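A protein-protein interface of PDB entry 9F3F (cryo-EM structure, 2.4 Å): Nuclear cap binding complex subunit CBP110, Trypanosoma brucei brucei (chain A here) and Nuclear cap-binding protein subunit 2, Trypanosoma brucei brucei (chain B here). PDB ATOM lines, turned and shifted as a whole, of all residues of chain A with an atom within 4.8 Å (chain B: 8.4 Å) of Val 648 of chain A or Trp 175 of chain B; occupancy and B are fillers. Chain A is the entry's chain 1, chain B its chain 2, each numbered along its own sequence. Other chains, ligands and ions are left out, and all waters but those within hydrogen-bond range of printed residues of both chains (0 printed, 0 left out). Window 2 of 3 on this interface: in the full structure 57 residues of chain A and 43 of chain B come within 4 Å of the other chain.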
ATOM      1  N   PRO A 564     -16.678   1.097   8.502  1.00  0.00           N
ATOM      2  CA  PRO A 564     -15.503   1.980   8.453  1.00  0.00           C
ATOM      3  C   PRO A 564     -14.310   1.356   7.758  1.00  0.00           C
ATOM      4  O   PRO A 564     -13.497   2.080   7.171  1.00  0.00           O
ATOM      5  CB  PRO A 564     -15.217   2.268   9.932  1.00  0.00           C
ATOM      6  CG  PRO A 564     -15.787   1.120  10.660  1.00  0.00           C
ATOM      7  CD  PRO A 564     -16.964   0.628   9.866  1.00  0.00           C
ATOM      8  N   SER A 565     -14.172   0.031   7.817  1.00  0.00           N
ATOM      9  CA  SER A 565     -13.099  -0.631   7.085  1.00  0.00           C
ATOM     10  C   SER A 565     -13.269  -0.462   5.582  1.00  0.00           C
ATOM     11  O   SER A 565     -12.293  -0.215   4.865  1.00  0.00           O
ATOM     12  CB  SER A 565     -13.052  -2.112   7.453  1.00  0.00           C
ATOM     13  OG  SER A 565     -14.201  -2.788   6.973  1.00  0.00           O
ATOM     14  N   THR A 641     -20.550   6.967  13.900  1.00  0.00           N
ATOM     15  CA  THR A 641     -19.578   6.538  14.894  1.00  0.00           C
ATOM     16  C   THR A 641     -20.123   6.677  16.308  1.00  0.00           C
ATOM     17  O   THR A 641     -19.721   5.921  17.198  1.00  0.00           O
ATOM     18  CB  THR A 641     -18.287   7.341  14.748  1.00  0.00           C
ATOM     19  OG1 THR A 641     -18.582   8.738  14.836  1.00  0.00           O
ATOM     20  CG2 THR A 641     -17.638   7.059  13.410  1.00  0.00           C
ATOM     21  N   THR A 645     -15.834   5.158  19.903  1.00  0.00           N
ATOM     22  CA  THR A 645     -14.582   4.428  19.761  1.00  0.00           C
ATOM     23  C   THR A 645     -13.575   5.328  19.061  1.00  0.00           C
ATOM     24  O   THR A 645     -13.824   5.787  17.942  1.00  0.00           O
ATOM     25  CB  THR A 645     -14.789   3.133  18.982  1.00  0.00           C
ATOM     26  OG1 THR A 645     -15.388   2.153  19.837  1.00  0.00           O
ATOM     27  CG2 THR A 645     -13.464   2.598  18.481  1.00  0.00           C
ATOM     28  N   VAL A 646     -12.452   5.619  19.705  1.00  0.00           N
ATOM     29  CA  VAL A 646     -11.426   6.524  19.105  1.00  0.00           C
ATOM     30  C   VAL A 646     -10.826   5.843  17.859  1.00  0.00           C
ATOM     31  O   VAL A 646     -10.468   6.556  16.925  1.00  0.00           O
ATOM     32  CB  VAL A 646     -10.334   6.965  20.096  1.00  0.00           C
ATOM     33  CG1 VAL A 646      -9.600   5.778  20.704  1.00  0.00           C
ATOM     34  CG2 VAL A 646      -9.357   7.956  19.482  1.00  0.00           C
ATOM     35  N   SER A 647     -10.731   4.517  17.846  1.00  0.00           N
ATOM     36  CA  SER A 647     -10.147   3.872  16.679  1.00  0.00           C
ATOM     37  C   SER A 647     -11.016   4.078  15.445  1.00  0.00           C
ATOM     38  O   SER A 647     -10.512   4.432  14.374  1.00  0.00           O
ATOM     39  CB  SER A 647      -9.935   2.384  16.954  1.00  0.00           C
ATOM     40  OG  SER A 647     -11.067   1.622  16.576  1.00  0.00           O
ATOM     41  N   VAL A 648     -12.328   3.870  15.580  1.00  0.00           N
ATOM     42  CA  VAL A 648     -13.233   4.064  14.448  1.00  0.00           C
ATOM     43  C   VAL A 648     -13.256   5.525  14.029  1.00  0.00           C
ATOM     44  O   VAL A 648     -13.221   5.845  12.835  1.00  0.00           O
ATOM     45  CB  VAL A 648     -14.641   3.552  14.794  1.00  0.00           C
ATOM     46  CG1 VAL A 648     -15.618   3.902  13.689  1.00  0.00           C
ATOM     47  CG2 VAL A 648     -14.612   2.066  15.013  1.00  0.00           C
ATOM     48  N   VAL A 649     -13.311   6.434  15.001  1.00  0.00           N
ATOM     49  CA  VAL A 649     -13.329   7.859  14.693  1.00  0.00           C
ATOM     50  C   VAL A 649     -12.069   8.253  13.937  1.00  0.00           C
ATOM     51  O   VAL A 649     -12.126   8.928  12.902  1.00  0.00           O
ATOM     52  CB  VAL A 649     -13.491   8.679  15.985  1.00  0.00           C
ATOM     53  CG1 VAL A 649     -12.997  10.083  15.786  1.00  0.00           C
ATOM     54  CG2 VAL A 649     -14.936   8.686  16.429  1.00  0.00           C
ATOM     55  N   GLN A 650     -10.909   7.820  14.436  1.00  0.00           N
ATOM     56  CA  GLN A 650      -9.650   8.179  13.797  1.00  0.00           C
ATOM     57  C   GLN A 650      -9.541   7.570  12.408  1.00  0.00           C
ATOM     58  O   GLN A 650      -9.116   8.242  11.467  1.00  0.00           O
ATOM     59  CB  GLN A 650      -8.475   7.748  14.672  1.00  0.00           C
ATOM     60  CG  GLN A 650      -7.854   8.880  15.462  1.00  0.00           C
ATOM     61  CD  GLN A 650      -6.543   8.490  16.104  1.00  0.00           C
ATOM     62  OE1 GLN A 650      -5.606   9.282  16.156  1.00  0.00           O
ATOM     63  NE2 GLN A 650      -6.470   7.262  16.598  1.00  0.00           N
ATOM     64  N   GLN A 651      -9.935   6.306  12.253  1.00  0.00           N
ATOM     65  CA  GLN A 651      -9.842   5.667  10.947  1.00  0.00           C
ATOM     66  C   GLN A 651     -10.761   6.337   9.933  1.00  0.00           C
ATOM     67  O   GLN A 651     -10.367   6.554   8.781  1.00  0.00           O
ATOM     68  CB  GLN A 651     -10.158   4.177  11.072  1.00  0.00           C
ATOM     69  CG  GLN A 651     -10.910   3.593   9.899  1.00  0.00           C
ATOM     70  CD  GLN A 651     -11.127   2.103  10.036  1.00  0.00           C
ATOM     71  OE1 GLN A 651     -12.154   1.659  10.544  1.00  0.00           O
ATOM     72  NE2 GLN A 651     -10.158   1.321   9.578  1.00  0.00           N
ATOM     73  N   LEU A 652     -11.982   6.685  10.340  1.00  0.00           N
ATOM     74  CA  LEU A 652     -12.902   7.333   9.414  1.00  0.00           C
ATOM     75  C   LEU A 652     -12.433   8.735   9.057  1.00  0.00           C
ATOM     76  O   LEU A 652     -12.538   9.151   7.898  1.00  0.00           O
ATOM     77  CB  LEU A 652     -14.307   7.360  10.005  1.00  0.00           C
ATOM     78  CG  LEU A 652     -15.117   6.094   9.743  1.00  0.00           C
ATOM     79  CD1 LEU A 652     -16.596   6.347   9.934  1.00  0.00           C
ATOM     80  CD2 LEU A 652     -14.837   5.583   8.352  1.00  0.00           C
ATOM     81  N   THR A 653     -11.904   9.476  10.030  1.00  0.00           N
ATOM     82  CA  THR A 653     -11.361  10.795   9.729  1.00  0.00           C
ATOM     83  C   THR A 653     -10.155  10.694   8.808  1.00  0.00           C
ATOM     84  O   THR A 653      -9.957  11.546   7.938  1.00  0.00           O
ATOM     85  CB  THR A 653     -10.986  11.519  11.018  1.00  0.00           C
ATOM     86  OG1 THR A 653     -12.068  11.428  11.951  1.00  0.00           O
ATOM     87  CG2 THR A 653     -10.692  12.976  10.738  1.00  0.00           C
ATOM     88  N   GLU B  55     -12.367   1.043  24.749  1.00  0.00           N
ATOM     89  CA  GLU B  55     -11.245   1.792  24.152  1.00  0.00           C
ATOM     90  C   GLU B  55     -11.144   3.165  24.803  1.00  0.00           C
ATOM     91  O   GLU B  55     -10.028   3.694  24.875  1.00  0.00           O
ATOM     92  CB  GLU B  55     -11.456   1.918  22.648  1.00  0.00           C
ATOM     93  CG  GLU B  55     -10.673   0.897  21.833  1.00  0.00           C
ATOM     94  CD  GLU B  55     -10.714   1.235  20.359  1.00  0.00           C
ATOM     95  OE1 GLU B  55     -10.303   2.364  20.023  1.00  0.00           O
ATOM     96  OE2 GLU B  55     -11.147   0.384  19.558  1.00  0.00           O
ATOM     97  N   LEU B  71      -4.827   2.962  18.107  1.00  0.00           N
ATOM     98  CA  LEU B  71      -5.130   2.102  19.275  1.00  0.00           C
ATOM     99  C   LEU B  71      -5.840   0.871  18.740  1.00  0.00           C
ATOM    100  O   LEU B  71      -6.982   1.001  18.295  1.00  0.00           O
ATOM    101  CB  LEU B  71      -6.001   2.828  20.297  1.00  0.00           C
ATOM    102  CG  LEU B  71      -6.103   2.222  21.698  1.00  0.00           C
ATOM    103  CD1 LEU B  71      -6.488   3.331  22.654  1.00  0.00           C
ATOM    104  CD2 LEU B  71      -7.145   1.124  21.739  1.00  0.00           C
ATOM    105  N   MET B  73      -7.259  -2.983  19.419  1.00  0.00           N
ATOM    106  CA  MET B  73      -7.716  -3.837  20.519  1.00  0.00           C
ATOM    107  C   MET B  73      -7.558  -5.282  20.101  1.00  0.00           C
ATOM    108  O   MET B  73      -7.931  -5.620  18.979  1.00  0.00           O
ATOM    109  CB  MET B  73      -9.195  -3.591  20.811  1.00  0.00           C
ATOM    110  CG  MET B  73      -9.652  -4.082  22.166  1.00  0.00           C
ATOM    111  SD  MET B  73      -9.364  -2.863  23.464  1.00  0.00           S
ATOM    112  CE  MET B  73     -11.040  -2.291  23.774  1.00  0.00           C
ATOM    113  N   LEU B  75      -8.528  -8.992  19.656  1.00  0.00           N
ATOM    114  CA  LEU B  75      -9.886  -9.465  19.370  1.00  0.00           C
ATOM    115  C   LEU B  75      -9.868 -10.972  19.186  1.00  0.00           C
ATOM    116  O   LEU B  75      -9.111 -11.446  18.329  1.00  0.00           O
ATOM    117  CB  LEU B  75     -10.314  -8.743  18.102  1.00  0.00           C
ATOM    118  CG  LEU B  75     -10.714  -7.272  18.250  1.00  0.00           C
ATOM    119  CD1 LEU B  75     -11.062  -6.691  16.897  1.00  0.00           C
ATOM    120  CD2 LEU B  75     -11.881  -7.123  19.204  1.00  0.00           C
ATOM    121  N   ARG B  80     -14.761 -11.873  17.748  1.00  0.00           N
ATOM    122  CA  ARG B  80     -14.366 -10.458  17.453  1.00  0.00           C
ATOM    123  C   ARG B  80     -14.611  -9.555  18.656  1.00  0.00           C
ATOM    124  O   ARG B  80     -14.859  -8.359  18.446  1.00  0.00           O
ATOM    125  CB  ARG B  80     -14.981  -9.893  16.169  1.00  0.00           C
ATOM    126  CG  ARG B  80     -14.482 -10.561  14.897  1.00  0.00           C
ATOM    127  CD  ARG B  80     -15.009  -9.869  13.655  1.00  0.00           C
ATOM    128  NE  ARG B  80     -16.458  -9.891  13.570  1.00  0.00           N
ATOM    129  CZ  ARG B  80     -17.159  -9.345  12.586  1.00  0.00           C
ATOM    130  NH1 ARG B  80     -16.542  -8.672  11.631  1.00  0.00           N
ATOM    131  NH2 ARG B  80     -18.475  -9.456  12.571  1.00  0.00           N
ATOM    132  N   PRO B  82     -13.055  -8.171  22.534  1.00  0.00           N
ATOM    133  CA  PRO B  82     -11.735  -7.995  23.148  1.00  0.00           C
ATOM    134  C   PRO B  82     -11.344  -9.221  23.955  1.00  0.00           C
ATOM    135  O   PRO B  82     -12.143  -9.771  24.715  1.00  0.00           O
ATOM    136  CB  PRO B  82     -11.924  -6.764  24.037  1.00  0.00           C
ATOM    137  CG  PRO B  82     -13.012  -6.011  23.380  1.00  0.00           C
ATOM    138  CD  PRO B  82     -13.957  -7.058  22.871  1.00  0.00           C
ATOM    139  N   HIS B 123      -2.560  -6.361  11.251  1.00  0.00           N
ATOM    140  CA  HIS B 123      -3.904  -6.927  11.496  1.00  0.00           C
ATOM    141  C   HIS B 123      -3.712  -8.302  12.136  1.00  0.00           C
ATOM    142  O   HIS B 123      -4.467  -8.658  13.066  1.00  0.00           O
ATOM    143  CB  HIS B 123      -4.716  -6.948  10.198  1.00  0.00           C
ATOM    144  CG  HIS B 123      -6.140  -7.361  10.368  1.00  0.00           C
ATOM    145  ND1 HIS B 123      -7.138  -6.471  10.702  1.00  0.00           N
ATOM    146  CD2 HIS B 123      -6.732  -8.556  10.258  1.00  0.00           C
ATOM    147  CE1 HIS B 123      -8.292  -7.118  10.783  1.00  0.00           C
ATOM    148  NE2 HIS B 123      -8.068  -8.385  10.515  1.00  0.00           N
ATOM    149  N   ARG B 126      -3.221  -8.236  15.906  1.00  0.00           N
ATOM    150  CA  ARG B 126      -4.399  -7.748  16.657  1.00  0.00           C
ATOM    151  C   ARG B 126      -5.248  -8.903  17.173  1.00  0.00           C
ATOM    152  O   ARG B 126      -6.126  -8.650  18.016  1.00  0.00           O
ATOM    153  CB  ARG B 126      -5.306  -6.927  15.737  1.00  0.00           C
ATOM    154  CG  ARG B 126      -6.494  -7.660  15.136  1.00  0.00           C
ATOM    155  CD  ARG B 126      -7.548  -6.721  14.589  1.00  0.00           C
ATOM    156  NE  ARG B 126      -8.141  -5.912  15.658  1.00  0.00           N
ATOM    157  CZ  ARG B 126      -8.159  -4.589  15.678  1.00  0.00           C
ATOM    158  NH1 ARG B 126      -7.698  -3.910  14.646  1.00  0.00           N
ATOM    159  NH2 ARG B 126      -8.643  -3.952  16.728  1.00  0.00           N
ATOM    160  N   TRP B 127      -5.020 -10.109  16.694  1.00  0.00           N
ATOM    161  CA  TRP B 127      -5.908 -11.221  17.085  1.00  0.00           C
ATOM    162  C   TRP B 127      -5.236 -12.075  18.140  1.00  0.00           C
ATOM    163  O   TRP B 127      -4.050 -11.849  18.424  1.00  0.00           O
ATOM    164  CB  TRP B 127      -6.289 -12.062  15.859  1.00  0.00           C
ATOM    165  CG  TRP B 127      -6.980 -11.295  14.767  1.00  0.00           C
ATOM    166  CD1 TRP B 127      -6.387 -10.655  13.721  1.00  0.00           C
ATOM    167  CD2 TRP B 127      -8.399 -11.085  14.609  1.00  0.00           C
ATOM    168  NE1 TRP B 127      -7.329 -10.051  12.935  1.00  0.00           N
ATOM    169  CE2 TRP B 127      -8.572 -10.299  13.451  1.00  0.00           C
ATOM    170  CE3 TRP B 127      -9.531 -11.476  15.329  1.00  0.00           C
ATOM    171  CZ2 TRP B 127      -9.828  -9.905  13.001  1.00  0.00           C
ATOM    172  CZ3 TRP B 127     -10.772 -11.087  14.883  1.00  0.00           C
ATOM    173  CH2 TRP B 127     -10.916 -10.311  13.736  1.00  0.00           C
ATOM    174  N   LEU B 170     -19.811  -6.520  26.411  1.00  0.00           N
ATOM    175  CA  LEU B 170     -18.836  -6.953  25.419  1.00  0.00           C
ATOM    176  C   LEU B 170     -19.011  -6.193  24.112  1.00  0.00           C
ATOM    177  O   LEU B 170     -20.020  -6.344  23.427  1.00  0.00           O
ATOM    178  CB  LEU B 170     -18.954  -8.457  25.172  1.00  0.00           C
ATOM    179  CG  LEU B 170     -18.124  -9.369  26.078  1.00  0.00           C
ATOM    180  CD1 LEU B 170     -18.154 -10.798  25.566  1.00  0.00           C
ATOM    181  CD2 LEU B 170     -16.697  -8.866  26.189  1.00  0.00           C
ATOM    182  N   VAL B 171     -18.019  -5.376  23.769  1.00  0.00           N
ATOM    183  CA  VAL B 171     -18.070  -4.590  22.539  1.00  0.00           C
ATOM    184  C   VAL B 171     -17.743  -5.511  21.370  1.00  0.00           C
ATOM    185  O   VAL B 171     -16.604  -5.961  21.221  1.00  0.00           O
ATOM    186  CB  VAL B 171     -17.108  -3.399  22.593  1.00  0.00           C
ATOM    187  CG1 VAL B 171     -17.315  -2.500  21.387  1.00  0.00           C
ATOM    188  CG2 VAL B 171     -17.297  -2.623  23.884  1.00  0.00           C
ATOM    189  N   HIS B 172     -18.741  -5.794  20.538  1.00  0.00           N
ATOM    190  CA  HIS B 172     -18.553  -6.638  19.361  1.00  0.00           C
ATOM    191  C   HIS B 172     -18.062  -5.761  18.221  1.00  0.00           C
ATOM    192  O   HIS B 172     -18.825  -4.981  17.647  1.00  0.00           O
ATOM    193  CB  HIS B 172     -19.852  -7.343  18.994  1.00  0.00           C
ATOM    194  CG  HIS B 172     -20.568  -7.934  20.166  1.00  0.00           C
ATOM    195  ND1 HIS B 172     -20.164  -9.103  20.772  1.00  0.00           N
ATOM    196  CD2 HIS B 172     -21.662  -7.516  20.845  1.00  0.00           C
ATOM    197  CE1 HIS B 172     -20.979  -9.380  21.775  1.00  0.00           C
ATOM    198  NE2 HIS B 172     -21.897  -8.432  21.841  1.00  0.00           N
ATOM    199  N   TYR B 173     -16.781  -5.887  17.881  1.00  0.00           N
ATOM    200  CA  TYR B 173     -16.192  -5.114  16.788  1.00  0.00           C
ATOM    201  C   TYR B 173     -16.653  -5.700  15.452  1.00  0.00           C
ATOM    202  O   TYR B 173     -15.875  -6.234  14.662  1.00  0.00           O
ATOM    203  CB  TYR B 173     -14.674  -5.100  16.881  1.00  0.00           C
ATOM    204  CG  TYR B 173     -14.092  -4.218  17.959  1.00  0.00           C
ATOM    205  CD1 TYR B 173     -14.585  -4.241  19.252  1.00  0.00           C
ATOM    206  CD2 TYR B 173     -13.041  -3.361  17.677  1.00  0.00           C
ATOM    207  CE1 TYR B 173     -14.047  -3.436  20.232  1.00  0.00           C
ATOM    208  CE2 TYR B 173     -12.500  -2.553  18.647  1.00  0.00           C
ATOM    209  CZ  TYR B 173     -13.005  -2.593  19.922  1.00  0.00           C
ATOM    210  OH  TYR B 173     -12.467  -1.786  20.890  1.00  0.00           O
ATOM    211  N   THR B 174     -17.956  -5.570  15.197  1.00  0.00           N
ATOM    212  CA  THR B 174     -18.514  -6.060  13.942  1.00  0.00           C
ATOM    213  C   THR B 174     -18.025  -5.267  12.739  1.00  0.00           C
ATOM    214  O   THR B 174     -18.252  -5.693  11.603  1.00  0.00           O
ATOM    215  CB  THR B 174     -20.040  -6.027  13.989  1.00  0.00           C
ATOM    216  OG1 THR B 174     -20.488  -4.680  14.181  1.00  0.00           O
ATOM    217  CG2 THR B 174     -20.555  -6.894  15.125  1.00  0.00           C
ATOM    218  N   TRP B 175     -17.368  -4.132  12.960  1.00  0.00           N
ATOM    219  CA  TRP B 175     -16.835  -3.310  11.886  1.00  0.00           C
ATOM    220  C   TRP B 175     -15.440  -3.724  11.441  1.00  0.00           C
ATOM    221  O   TRP B 175     -14.951  -3.204  10.432  1.00  0.00           O
ATOM    222  CB  TRP B 175     -16.814  -1.847  12.319  1.00  0.00           C
ATOM    223  CG  TRP B 175     -16.134  -1.607  13.623  1.00  0.00           C
ATOM    224  CD1 TRP B 175     -14.812  -1.352  13.823  1.00  0.00           C
ATOM    225  CD2 TRP B 175     -16.745  -1.596  14.915  1.00  0.00           C
ATOM    226  NE1 TRP B 175     -14.561  -1.181  15.162  1.00  0.00           N
ATOM    227  CE2 TRP B 175     -15.734  -1.325  15.854  1.00  0.00           C
ATOM    228  CE3 TRP B 175     -18.052  -1.788  15.369  1.00  0.00           C
ATOM    229  CZ2 TRP B 175     -15.986  -1.244  17.218  1.00  0.00           C
ATOM    230  CZ3 TRP B 175     -18.301  -1.705  16.723  1.00  0.00           C
ATOM    231  CH2 TRP B 175     -17.274  -1.436  17.633  1.00  0.00           C
ATOM    232  N   ILE B 176     -14.774  -4.591  12.206  1.00  0.00           N
ATOM    233  CA  ILE B 176     -13.421  -5.083  11.810  1.00  0.00           C
ATOM    234  C   ILE B 176     -13.598  -6.356  10.970  1.00  0.00           C
ATOM    235  O   ILE B 176     -14.242  -7.302  11.463  1.00  0.00           O
ATOM    236  CB  ILE B 176     -12.527  -5.313  13.040  1.00  0.00           C
ATOM    237  CG1 ILE B 176     -12.147  -3.997  13.702  1.00  0.00           C
ATOM    238  CG2 ILE B 176     -11.288  -6.132  12.674  1.00  0.00           C
ATOM    239  CD1 ILE B 176     -11.313  -3.087  12.822  1.00  0.00           C
ATOM    240  N   PRO B 177     -13.080  -6.407   9.720  1.00  0.00           N
ATOM    241  CA  PRO B 177     -13.247  -7.573   8.856  1.00  0.00           C
ATOM    242  C   PRO B 177     -12.558  -8.786   9.452  1.00  0.00           C
ATOM    243  O   PRO B 177     -11.364  -8.731   9.783  1.00  0.00           O
ATOM    244  CB  PRO B 177     -12.579  -7.137   7.545  1.00  0.00           C
ATOM    245  CG  PRO B 177     -11.589  -6.109   7.959  1.00  0.00           C
ATOM    246  CD  PRO B 177     -12.205  -5.388   9.116  1.00  0.00           C
ATOM    247  N   PRO B 178     -13.276  -9.893   9.617  1.00  0.00           N
ATOM    248  CA  PRO B 178     -12.655 -11.090  10.195  1.00  0.00           C
ATOM    249  C   PRO B 178     -11.518 -11.599   9.323  1.00  0.00           C
ATOM    250  O   PRO B 178     -11.585 -11.557   8.093  1.00  0.00           O
ATOM    251  CB  PRO B 178     -13.811 -12.094  10.265  1.00  0.00           C
ATOM    252  CG  PRO B 178     -14.811 -11.604   9.277  1.00  0.00           C
ATOM    253  CD  PRO B 178     -14.687 -10.111   9.266  1.00  0.00           C
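The side-chain carboxylate (OE1) of Glu 55 of chain B sits close to the backbone NH (N) of Ser 647 of chain A, 3.1 Å away.
Of the printed residues of chain B, Pro 564 of chain A touches Trp 175 (3.5 Å).
Of the printed residues of chain B, Thr 645 of chain A touches Glu 55 (3.4 Å).
Of the printed residues of chain B, Val 646 of chain A touches Glu 55 (3.6 Å).
Of chain B, only Glu 55 and Leu 71 come within 4 Å of Ser 647 of chain A.
Of the printed residues of chain B, Val 648 of chain A touches Trp 175.
Trp 175 of chain B touches three residues of chain A.
The nearest printed residue of chain B that does not touch Ser 565 of chain A is Ile 176 of chain B (5.3 Å).
Of the 12 printed residues of chain A, 6 touch a printed residue of chain B.
Hydrophobic or aromatic side chains of chain A within 4 Å of the printed part of chain B: Pro 564, Val 646 and Val 648.
Along chain A the printed residues that touch a printed residue of chain B span positions 564 to 648.
Of the 18 printed residues of chain B, 4 touch a printed residue of chain A.
Among the printed residues, no Asp or Glu carboxylate lies within 4 Å of a Lys or Arg side-chain nitrogen of the other chain.
The side-chain hydroxyl (OH) of Tyr 173 of chain B lies within hydrogen-bond range of the side-chain carboxylate (OE2) of Glu 55 of chain B, 2.9 Å away.
NE2 of His 123 of chain B is in hydrogen-bond range of O of Pro 177 of chain B, 3.4 Å away.
Among the printed residues, merely in contact across the chains: Val 648 of chain A with Trp 175 of chain B (3.3 Å), Thr 645 of chain A with Glu 55 of chain B (3.4 Å), Pro 564 of chain A with Trp 175 of chain B (3.5 Å), Ser 647 of chain A with Leu 71 of chain B (3.5 Å), Val 646 of chain A with Glu 55 of chain B (3.6 Å), Ser 565 of chain A with Trp 175 of chain B (3.6 Å) and Ser 565 of chain A with Pro 177 of chain B (3.8 Å).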
